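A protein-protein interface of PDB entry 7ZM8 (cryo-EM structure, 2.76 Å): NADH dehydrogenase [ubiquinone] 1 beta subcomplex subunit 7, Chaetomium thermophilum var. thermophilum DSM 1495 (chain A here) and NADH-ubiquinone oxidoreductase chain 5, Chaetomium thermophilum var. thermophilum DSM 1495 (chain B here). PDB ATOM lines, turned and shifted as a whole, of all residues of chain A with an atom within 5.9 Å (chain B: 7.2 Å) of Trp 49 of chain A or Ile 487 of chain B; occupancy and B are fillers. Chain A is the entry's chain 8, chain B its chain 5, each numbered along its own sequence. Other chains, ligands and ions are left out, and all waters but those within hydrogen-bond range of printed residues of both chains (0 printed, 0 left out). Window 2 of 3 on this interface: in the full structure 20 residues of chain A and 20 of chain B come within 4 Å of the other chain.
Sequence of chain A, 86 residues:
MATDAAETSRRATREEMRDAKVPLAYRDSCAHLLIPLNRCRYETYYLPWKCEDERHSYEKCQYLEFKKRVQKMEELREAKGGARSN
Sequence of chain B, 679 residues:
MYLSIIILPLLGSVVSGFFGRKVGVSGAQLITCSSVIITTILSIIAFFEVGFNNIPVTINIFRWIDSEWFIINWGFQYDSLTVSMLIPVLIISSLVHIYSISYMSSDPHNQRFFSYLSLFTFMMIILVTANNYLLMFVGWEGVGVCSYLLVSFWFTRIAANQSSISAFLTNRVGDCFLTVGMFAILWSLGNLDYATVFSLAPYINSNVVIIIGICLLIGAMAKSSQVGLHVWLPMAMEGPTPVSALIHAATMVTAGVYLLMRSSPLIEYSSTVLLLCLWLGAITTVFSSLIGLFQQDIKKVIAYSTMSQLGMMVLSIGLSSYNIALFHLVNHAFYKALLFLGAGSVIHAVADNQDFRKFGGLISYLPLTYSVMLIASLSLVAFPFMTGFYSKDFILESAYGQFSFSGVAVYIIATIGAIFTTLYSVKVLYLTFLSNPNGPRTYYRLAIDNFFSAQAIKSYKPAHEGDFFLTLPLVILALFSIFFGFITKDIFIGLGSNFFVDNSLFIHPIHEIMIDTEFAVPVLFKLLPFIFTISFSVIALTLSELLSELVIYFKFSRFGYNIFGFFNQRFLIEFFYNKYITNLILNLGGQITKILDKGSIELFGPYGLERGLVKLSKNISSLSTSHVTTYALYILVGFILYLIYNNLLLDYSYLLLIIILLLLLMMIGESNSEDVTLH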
ATOM      1  N   TYR A  46     -27.438 -28.101  -1.735  1.00  0.00           N
ATOM      2  CA  TYR A  46     -26.826 -26.795  -1.472  1.00  0.00           C
ATOM      3  C   TYR A  46     -26.220 -26.172  -2.723  1.00  0.00           C
ATOM      4  O   TYR A  46     -25.259 -25.406  -2.639  1.00  0.00           O
ATOM      5  CB  TYR A  46     -25.760 -26.879  -0.376  1.00  0.00           C
ATOM      6  CG  TYR A  46     -26.279 -27.248   0.983  1.00  0.00           C
ATOM      7  CD1 TYR A  46     -26.529 -28.568   1.315  1.00  0.00           C
ATOM      8  CD2 TYR A  46     -26.524 -26.275   1.935  1.00  0.00           C
ATOM      9  CE1 TYR A  46     -27.005 -28.909   2.557  1.00  0.00           C
ATOM     10  CE2 TYR A  46     -26.999 -26.605   3.183  1.00  0.00           C
ATOM     11  CZ  TYR A  46     -27.236 -27.925   3.490  1.00  0.00           C
ATOM     12  OH  TYR A  46     -27.713 -28.260   4.732  1.00  0.00           O
ATOM     13  N   LEU A  47     -26.755 -26.486  -3.887  1.00  0.00           N
ATOM     14  CA  LEU A  47     -26.269 -25.843  -5.097  1.00  0.00           C
ATOM     15  C   LEU A  47     -26.734 -24.393  -5.104  1.00  0.00           C
ATOM     16  O   LEU A  47     -27.929 -24.132  -4.949  1.00  0.00           O
ATOM     17  CB  LEU A  47     -26.751 -26.568  -6.347  1.00  0.00           C
ATOM     18  CG  LEU A  47     -25.943 -27.792  -6.787  1.00  0.00           C
ATOM     19  CD1 LEU A  47     -24.540 -27.373  -7.162  1.00  0.00           C
ATOM     20  CD2 LEU A  47     -25.899 -28.903  -5.764  1.00  0.00           C
ATOM     21  N   PRO A  48     -25.831 -23.428  -5.270  1.00  0.00           N
ATOM     22  CA  PRO A  48     -26.185 -22.021  -5.058  1.00  0.00           C
ATOM     23  C   PRO A  48     -27.069 -21.408  -6.131  1.00  0.00           C
ATOM     24  O   PRO A  48     -27.290 -20.196  -6.095  1.00  0.00           O
ATOM     25  CB  PRO A  48     -24.813 -21.329  -5.027  1.00  0.00           C
ATOM     26  CG  PRO A  48     -23.918 -22.224  -5.774  1.00  0.00           C
ATOM     27  CD  PRO A  48     -24.394 -23.608  -5.531  1.00  0.00           C
ATOM     28  N   TRP A  49     -27.593 -22.189  -7.074  1.00  0.00           N
ATOM     29  CA  TRP A  49     -28.466 -21.647  -8.106  1.00  0.00           C
ATOM     30  C   TRP A  49     -29.772 -22.417  -8.229  1.00  0.00           C
ATOM     31  O   TRP A  49     -30.391 -22.397  -9.296  1.00  0.00           O
ATOM     32  CB  TRP A  49     -27.761 -21.632  -9.458  1.00  0.00           C
ATOM     33  CG  TRP A  49     -27.341 -22.980  -9.897  1.00  0.00           C
ATOM     34  CD1 TRP A  49     -28.096 -23.899 -10.555  1.00  0.00           C
ATOM     35  CD2 TRP A  49     -26.061 -23.573  -9.708  1.00  0.00           C
ATOM     36  NE1 TRP A  49     -27.365 -25.032 -10.790  1.00  0.00           N
ATOM     37  CE2 TRP A  49     -26.109 -24.855 -10.279  1.00  0.00           C
ATOM     38  CE3 TRP A  49     -24.874 -23.142  -9.112  1.00  0.00           C
ATOM     39  CZ2 TRP A  49     -25.016 -25.710 -10.276  1.00  0.00           C
ATOM     40  CZ3 TRP A  49     -23.793 -23.990  -9.106  1.00  0.00           C
ATOM     41  CH2 TRP A  49     -23.868 -25.258  -9.689  1.00  0.00           C
ATOM     42  N   LYS A  50     -30.213 -23.092  -7.177  1.00  0.00           N
ATOM     43  CA  LYS A  50     -31.399 -23.923  -7.295  1.00  0.00           C
ATOM     44  C   LYS A  50     -32.516 -23.557  -6.325  1.00  0.00           C
ATOM     45  O   LYS A  50     -33.682 -23.814  -6.631  1.00  0.00           O
ATOM     46  CB  LYS A  50     -31.023 -25.403  -7.117  1.00  0.00           C
ATOM     47  CG  LYS A  50     -32.160 -26.370  -7.388  1.00  0.00           C
ATOM     48  CD  LYS A  50     -32.648 -26.264  -8.822  1.00  0.00           C
ATOM     49  CE  LYS A  50     -31.588 -26.722  -9.808  1.00  0.00           C
ATOM     50  NZ  LYS A  50     -31.346 -28.188  -9.715  1.00  0.00           N
ATOM     51  N   CYS A  51     -32.205 -22.943  -5.187  1.00  0.00           N
ATOM     52  CA  CYS A  51     -33.212 -22.551  -4.208  1.00  0.00           C
ATOM     53  C   CYS A  51     -33.268 -21.036  -4.063  1.00  0.00           C
ATOM     54  O   CYS A  51     -33.384 -20.505  -2.960  1.00  0.00           O
ATOM     55  CB  CYS A  51     -32.941 -23.212  -2.859  1.00  0.00           C
ATOM     56  SG  CYS A  51     -33.104 -25.005  -2.889  1.00  0.00           S
ATOM     57  N   GLU A  52     -33.120 -20.339  -5.207  1.00  0.00           N
ATOM     58  CA  GLU A  52     -33.007 -18.854  -5.170  1.00  0.00           C
ATOM     59  C   GLU A  52     -34.198 -18.179  -4.487  1.00  0.00           C
ATOM     60  O   GLU A  52     -33.952 -17.292  -3.653  1.00  0.00           O
ATOM     61  CB  GLU A  52     -32.755 -18.296  -6.574  1.00  0.00           C
ATOM     62  CG  GLU A  52     -33.914 -18.463  -7.545  1.00  0.00           C
ATOM     63  CD  GLU A  52     -34.153 -19.869  -8.072  1.00  0.00           C
ATOM     64  OE1 GLU A  52     -33.181 -20.646  -8.145  1.00  0.00           O
ATOM     65  OE2 GLU A  52     -35.313 -20.185  -8.399  1.00  0.00           O
ATOM     66  N   ARG A  55     -34.159 -18.548  -0.571  1.00  0.00           N
ATOM     67  CA  ARG A  55     -33.140 -17.708   0.046  1.00  0.00           C
ATOM     68  C   ARG A  55     -33.579 -16.256   0.061  1.00  0.00           C
ATOM     69  O   ARG A  55     -33.426 -15.563   1.071  1.00  0.00           O
ATOM     70  CB  ARG A  55     -31.809 -17.840  -0.684  1.00  0.00           C
ATOM     71  CG  ARG A  55     -31.363 -19.249  -0.925  1.00  0.00           C
ATOM     72  CD  ARG A  55     -30.179 -19.297  -1.863  1.00  0.00           C
ATOM     73  NE  ARG A  55     -29.793 -20.672  -2.146  1.00  0.00           N
ATOM     74  CZ  ARG A  55     -29.164 -21.455  -1.280  1.00  0.00           C
ATOM     75  NH1 ARG A  55     -28.850 -22.697  -1.612  1.00  0.00           N
ATOM     76  NH2 ARG A  55     -28.850 -20.992  -0.083  1.00  0.00           N
ATOM     77  N   PHE B  52     -24.225 -34.364   3.715  1.00  0.00           N
ATOM     78  CA  PHE B  52     -25.422 -33.988   2.974  1.00  0.00           C
ATOM     79  C   PHE B  52     -26.665 -34.672   3.516  1.00  0.00           C
ATOM     80  O   PHE B  52     -27.783 -34.278   3.175  1.00  0.00           O
ATOM     81  CB  PHE B  52     -25.239 -34.311   1.496  1.00  0.00           C
ATOM     82  CG  PHE B  52     -24.463 -33.272   0.752  1.00  0.00           C
ATOM     83  CD1 PHE B  52     -24.846 -31.947   0.792  1.00  0.00           C
ATOM     84  CD2 PHE B  52     -23.345 -33.616   0.025  1.00  0.00           C
ATOM     85  CE1 PHE B  52     -24.134 -30.993   0.117  1.00  0.00           C
ATOM     86  CE2 PHE B  52     -22.634 -32.662  -0.658  1.00  0.00           C
ATOM     87  CZ  PHE B  52     -23.028 -31.350  -0.610  1.00  0.00           C
ATOM     88  N   PHE B 327     -14.211 -22.740   5.975  1.00  0.00           N
ATOM     89  CA  PHE B 327     -14.282 -22.419   4.554  1.00  0.00           C
ATOM     90  C   PHE B 327     -12.933 -21.944   4.030  1.00  0.00           C
ATOM     91  O   PHE B 327     -12.496 -22.348   2.949  1.00  0.00           O
ATOM     92  CB  PHE B 327     -15.352 -21.357   4.327  1.00  0.00           C
ATOM     93  CG  PHE B 327     -15.747 -21.190   2.898  1.00  0.00           C
ATOM     94  CD1 PHE B 327     -15.851 -22.284   2.064  1.00  0.00           C
ATOM     95  CD2 PHE B 327     -16.022 -19.940   2.388  1.00  0.00           C
ATOM     96  CE1 PHE B 327     -16.223 -22.130   0.756  1.00  0.00           C
ATOM     97  CE2 PHE B 327     -16.395 -19.784   1.075  1.00  0.00           C
ATOM     98  CZ  PHE B 327     -16.492 -20.876   0.259  1.00  0.00           C
ATOM     99  N   THR B 387     -11.905 -18.470  -5.725  1.00  0.00           N
ATOM    100  CA  THR B 387     -12.194 -19.315  -4.574  1.00  0.00           C
ATOM    101  C   THR B 387     -11.833 -18.611  -3.273  1.00  0.00           C
ATOM    102  O   THR B 387     -12.595 -18.660  -2.301  1.00  0.00           O
ATOM    103  CB  THR B 387     -11.457 -20.647  -4.706  1.00  0.00           C
ATOM    104  OG1 THR B 387     -12.021 -21.390  -5.791  1.00  0.00           O
ATOM    105  CG2 THR B 387     -11.592 -21.468  -3.449  1.00  0.00           C
ATOM    106  N   TYR B 390     -14.360 -15.628  -1.580  1.00  0.00           N
ATOM    107  CA  TYR B 390     -15.475 -15.870  -0.678  1.00  0.00           C
ATOM    108  C   TYR B 390     -15.028 -16.229   0.725  1.00  0.00           C
ATOM    109  O   TYR B 390     -15.823 -16.119   1.663  1.00  0.00           O
ATOM    110  CB  TYR B 390     -16.373 -16.973  -1.237  1.00  0.00           C
ATOM    111  CG  TYR B 390     -16.966 -16.612  -2.570  1.00  0.00           C
ATOM    112  CD1 TYR B 390     -16.304 -16.912  -3.746  1.00  0.00           C
ATOM    113  CD2 TYR B 390     -18.190 -15.976  -2.649  1.00  0.00           C
ATOM    114  CE1 TYR B 390     -16.839 -16.578  -4.966  1.00  0.00           C
ATOM    115  CE2 TYR B 390     -18.731 -15.633  -3.863  1.00  0.00           C
ATOM    116  CZ  TYR B 390     -18.056 -15.941  -5.022  1.00  0.00           C
ATOM    117  OH  TYR B 390     -18.602 -15.607  -6.238  1.00  0.00           O
ATOM    118  N   PHE B 480     -10.000 -26.141  -9.227  1.00  0.00           N
ATOM    119  CA  PHE B 480     -10.456 -25.894  -7.863  1.00  0.00           C
ATOM    120  C   PHE B 480     -10.291 -24.430  -7.486  1.00  0.00           C
ATOM    121  O   PHE B 480     -11.203 -23.819  -6.920  1.00  0.00           O
ATOM    122  CB  PHE B 480      -9.684 -26.770  -6.884  1.00  0.00           C
ATOM    123  CG  PHE B 480     -10.274 -28.128  -6.686  1.00  0.00           C
ATOM    124  CD1 PHE B 480     -11.388 -28.303  -5.893  1.00  0.00           C
ATOM    125  CD2 PHE B 480      -9.696 -29.236  -7.271  1.00  0.00           C
ATOM    126  CE1 PHE B 480     -11.923 -29.550  -5.701  1.00  0.00           C
ATOM    127  CE2 PHE B 480     -10.227 -30.490  -7.081  1.00  0.00           C
ATOM    128  CZ  PHE B 480     -11.344 -30.647  -6.294  1.00  0.00           C
ATOM    129  N   ILE B 482     -10.477 -21.835  -9.108  1.00  0.00           N
ATOM    130  CA  ILE B 482     -11.375 -20.919  -9.792  1.00  0.00           C
ATOM    131  C   ILE B 482     -12.813 -21.082  -9.320  1.00  0.00           C
ATOM    132  O   ILE B 482     -13.537 -20.096  -9.184  1.00  0.00           O
ATOM    133  CB  ILE B 482     -11.275 -21.102 -11.321  1.00  0.00           C
ATOM    134  CG1 ILE B 482      -9.839 -20.909 -11.798  1.00  0.00           C
ATOM    135  CG2 ILE B 482     -12.186 -20.121 -12.034  1.00  0.00           C
ATOM    136  CD1 ILE B 482      -9.671 -21.109 -13.275  1.00  0.00           C
ATOM    137  N   PHE B 483     -13.241 -22.314  -9.046  1.00  0.00           N
ATOM    138  CA  PHE B 483     -14.657 -22.607  -8.907  1.00  0.00           C
ATOM    139  C   PHE B 483     -15.073 -23.182  -7.563  1.00  0.00           C
ATOM    140  O   PHE B 483     -16.260 -23.119  -7.238  1.00  0.00           O
ATOM    141  CB  PHE B 483     -15.096 -23.586 -10.002  1.00  0.00           C
ATOM    142  CG  PHE B 483     -14.818 -23.097 -11.385  1.00  0.00           C
ATOM    143  CD1 PHE B 483     -15.496 -22.010 -11.895  1.00  0.00           C
ATOM    144  CD2 PHE B 483     -13.870 -23.714 -12.170  1.00  0.00           C
ATOM    145  CE1 PHE B 483     -15.240 -21.556 -13.164  1.00  0.00           C
ATOM    146  CE2 PHE B 483     -13.610 -23.263 -13.439  1.00  0.00           C
ATOM    147  CZ  PHE B 483     -14.297 -22.184 -13.936  1.00  0.00           C
ATOM    148  N   PHE B 484     -14.149 -23.734  -6.776  1.00  0.00           N
ATOM    149  CA  PHE B 484     -14.559 -24.471  -5.588  1.00  0.00           C
ATOM    150  C   PHE B 484     -15.229 -23.567  -4.564  1.00  0.00           C
ATOM    151  O   PHE B 484     -16.116 -24.016  -3.832  1.00  0.00           O
ATOM    152  CB  PHE B 484     -13.360 -25.181  -4.967  1.00  0.00           C
ATOM    153  CG  PHE B 484     -13.680 -25.901  -3.700  1.00  0.00           C
ATOM    154  CD1 PHE B 484     -14.269 -27.149  -3.736  1.00  0.00           C
ATOM    155  CD2 PHE B 484     -13.384 -25.342  -2.475  1.00  0.00           C
ATOM    156  CE1 PHE B 484     -14.566 -27.821  -2.575  1.00  0.00           C
ATOM    157  CE2 PHE B 484     -13.688 -26.007  -1.307  1.00  0.00           C
ATOM    158  CZ  PHE B 484     -14.277 -27.249  -1.358  1.00  0.00           C
ATOM    159  N   GLY B 485     -14.817 -22.301  -4.489  1.00  0.00           N
ATOM    160  CA  GLY B 485     -15.442 -21.390  -3.544  1.00  0.00           C
ATOM    161  C   GLY B 485     -16.903 -21.139  -3.857  1.00  0.00           C
ATOM    162  O   GLY B 485     -17.757 -21.174  -2.971  1.00  0.00           O
ATOM    163  N   PHE B 486     -17.208 -20.881  -5.128  1.00  0.00           N
ATOM    164  CA  PHE B 486     -18.591 -20.637  -5.522  1.00  0.00           C
ATOM    165  C   PHE B 486     -19.462 -21.860  -5.279  1.00  0.00           C
ATOM    166  O   PHE B 486     -20.585 -21.743  -4.780  1.00  0.00           O
ATOM    167  CB  PHE B 486     -18.653 -20.231  -6.994  1.00  0.00           C
ATOM    168  CG  PHE B 486     -20.022 -19.845  -7.456  1.00  0.00           C
ATOM    169  CD1 PHE B 486     -20.909 -20.797  -7.921  1.00  0.00           C
ATOM    170  CD2 PHE B 486     -20.422 -18.527  -7.433  1.00  0.00           C
ATOM    171  CE1 PHE B 486     -22.166 -20.440  -8.342  1.00  0.00           C
ATOM    172  CE2 PHE B 486     -21.679 -18.166  -7.851  1.00  0.00           C
ATOM    173  CZ  PHE B 486     -22.551 -19.125  -8.307  1.00  0.00           C
ATOM    174  N   ILE B 487     -18.957 -23.045  -5.624  1.00  0.00           N
ATOM    175  CA  ILE B 487     -19.792 -24.235  -5.640  1.00  0.00           C
ATOM    176  C   ILE B 487     -20.081 -24.730  -4.232  1.00  0.00           C
ATOM    177  O   ILE B 487     -20.983 -25.551  -4.039  1.00  0.00           O
ATOM    178  CB  ILE B 487     -19.118 -25.316  -6.508  1.00  0.00           C
ATOM    179  CG1 ILE B 487     -20.086 -26.452  -6.816  1.00  0.00           C
ATOM    180  CG2 ILE B 487     -17.883 -25.859  -5.834  1.00  0.00           C
ATOM    181  CD1 ILE B 487     -21.229 -26.030  -7.674  1.00  0.00           C
ATOM    182  N   THR B 488     -19.359 -24.227  -3.232  1.00  0.00           N
ATOM    183  CA  THR B 488     -19.514 -24.660  -1.850  1.00  0.00           C
ATOM    184  C   THR B 488     -19.810 -23.518  -0.887  1.00  0.00           C
ATOM    185  O   THR B 488     -19.793 -23.733   0.329  1.00  0.00           O
ATOM    186  CB  THR B 488     -18.255 -25.400  -1.391  1.00  0.00           C
ATOM    187  OG1 THR B 488     -17.155 -24.486  -1.349  1.00  0.00           O
ATOM    188  CG2 THR B 488     -17.922 -26.541  -2.328  1.00  0.00           C
ATOM    189  N   LYS B 489     -20.115 -22.318  -1.452  1.00  0.00           N
ATOM    190  CA  LYS B 489     -20.331 -21.128  -0.583  1.00  0.00           C
ATOM    191  C   LYS B 489     -21.539 -21.355   0.341  1.00  0.00           C
ATOM    192  O   LYS B 489     -21.493 -20.883   1.474  1.00  0.00           O
ATOM    193  CB  LYS B 489     -20.444 -19.837  -1.401  1.00  0.00           C
ATOM    194  CG  LYS B 489     -21.569 -19.804  -2.427  1.00  0.00           C
ATOM    195  CD  LYS B 489     -22.497 -18.622  -2.270  1.00  0.00           C
ATOM    196  CE  LYS B 489     -21.794 -17.292  -2.436  1.00  0.00           C
ATOM    197  NZ  LYS B 489     -22.731 -16.154  -2.289  1.00  0.00           N
ATOM    198  N   ASP B 490     -22.548 -22.075  -0.089  1.00  0.00           N
ATOM    199  CA  ASP B 490     -23.744 -22.321   0.703  1.00  0.00           C
ATOM    200  C   ASP B 490     -23.501 -23.328   1.816  1.00  0.00           C
ATOM    201  O   ASP B 490     -24.036 -23.169   2.916  1.00  0.00           O
ATOM    202  CB  ASP B 490     -24.868 -22.804  -0.205  1.00  0.00           C
ATOM    203  CG  ASP B 490     -26.225 -22.553   0.379  1.00  0.00           C
ATOM    204  OD1 ASP B 490     -26.405 -21.487   0.998  1.00  0.00           O
ATOM    205  OD2 ASP B 490     -27.107 -23.416   0.221  1.00  0.00           O
ATOM    206  N   ILE B 491     -22.706 -24.365   1.549  1.00  0.00           N
ATOM    207  CA  ILE B 491     -22.414 -25.380   2.556  1.00  0.00           C
ATOM    208  C   ILE B 491     -21.719 -24.765   3.761  1.00  0.00           C
ATOM    209  O   ILE B 491     -21.865 -25.251   4.888  1.00  0.00           O
ATOM    210  CB  ILE B 491     -21.566 -26.500   1.922  1.00  0.00           C
ATOM    211  CG1 ILE B 491     -22.351 -27.193   0.817  1.00  0.00           C
ATOM    212  CG2 ILE B 491     -21.139 -27.518   2.954  1.00  0.00           C
ATOM    213  CD1 ILE B 491     -21.514 -28.113  -0.019  1.00  0.00           C
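Of the printed residues of chain B, Tyr 46 of chain A touches Phe 52, Asp 490 and Ile 491. Thr 387 of chain B touches none of the printed residues of chain A. Lys 489 of chain B touches none of the printed residues of chain A. Of the printed residues of chain A, Asp 490 of chain B touches Tyr 46 and Arg 55. The nearest printed residue of chain B that does not touch Leu 47 of chain A is Asp 490 of chain B (5.1 Å).
NH1 of Arg 55 of chain A lies within salt-bridge range of OD2 of Asp 490 of chain B.
Phe 52 of chain B touches Tyr 46 of chain A. CD2 of Tyr 46 of chain A touches OD2 of Asp 490 of chain B, 3.4 Å away. CB of Tyr 46 of chain A touches CG1 of Ile 491 of chain B (3.6 Å). CD1 of Ile 487 of chain B touches CD1 of Leu 47 of chain A, 3.6 Å away. CG of Pro 48 of chain A touches O of Phe 486 of chain B, 3.5 Å away. Trp 49 of chain A touches Phe 486 of chain B (CE3 to CE1, 3.9 Å). Trp 49 of chain A touches Ile 487 of chain B (CH2 to CD1, 3.4 Å).
Of the 15 printed residues of chain B, 5 touch a printed residue of chain A. Hydrophobic or aromatic side chains of chain B that line the printed part of chain A: Phe 52, Phe 486, Ile 487 and Ile 491. Of the 8 printed residues of chain A, 5 touch a printed residue of chain B. Hydrophobic or aromatic side chains of chain A within 4 Å of the printed part of chain B: Tyr 46, Leu 47, Pro 48 and Trp 49. Among the printed residues, Asp or Glu carboxylates within 4 Å of a Lys or Arg side-chain nitrogen of the other chain: Arg 55 of chain A with Asp 490 of chain B (2.6 Å).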
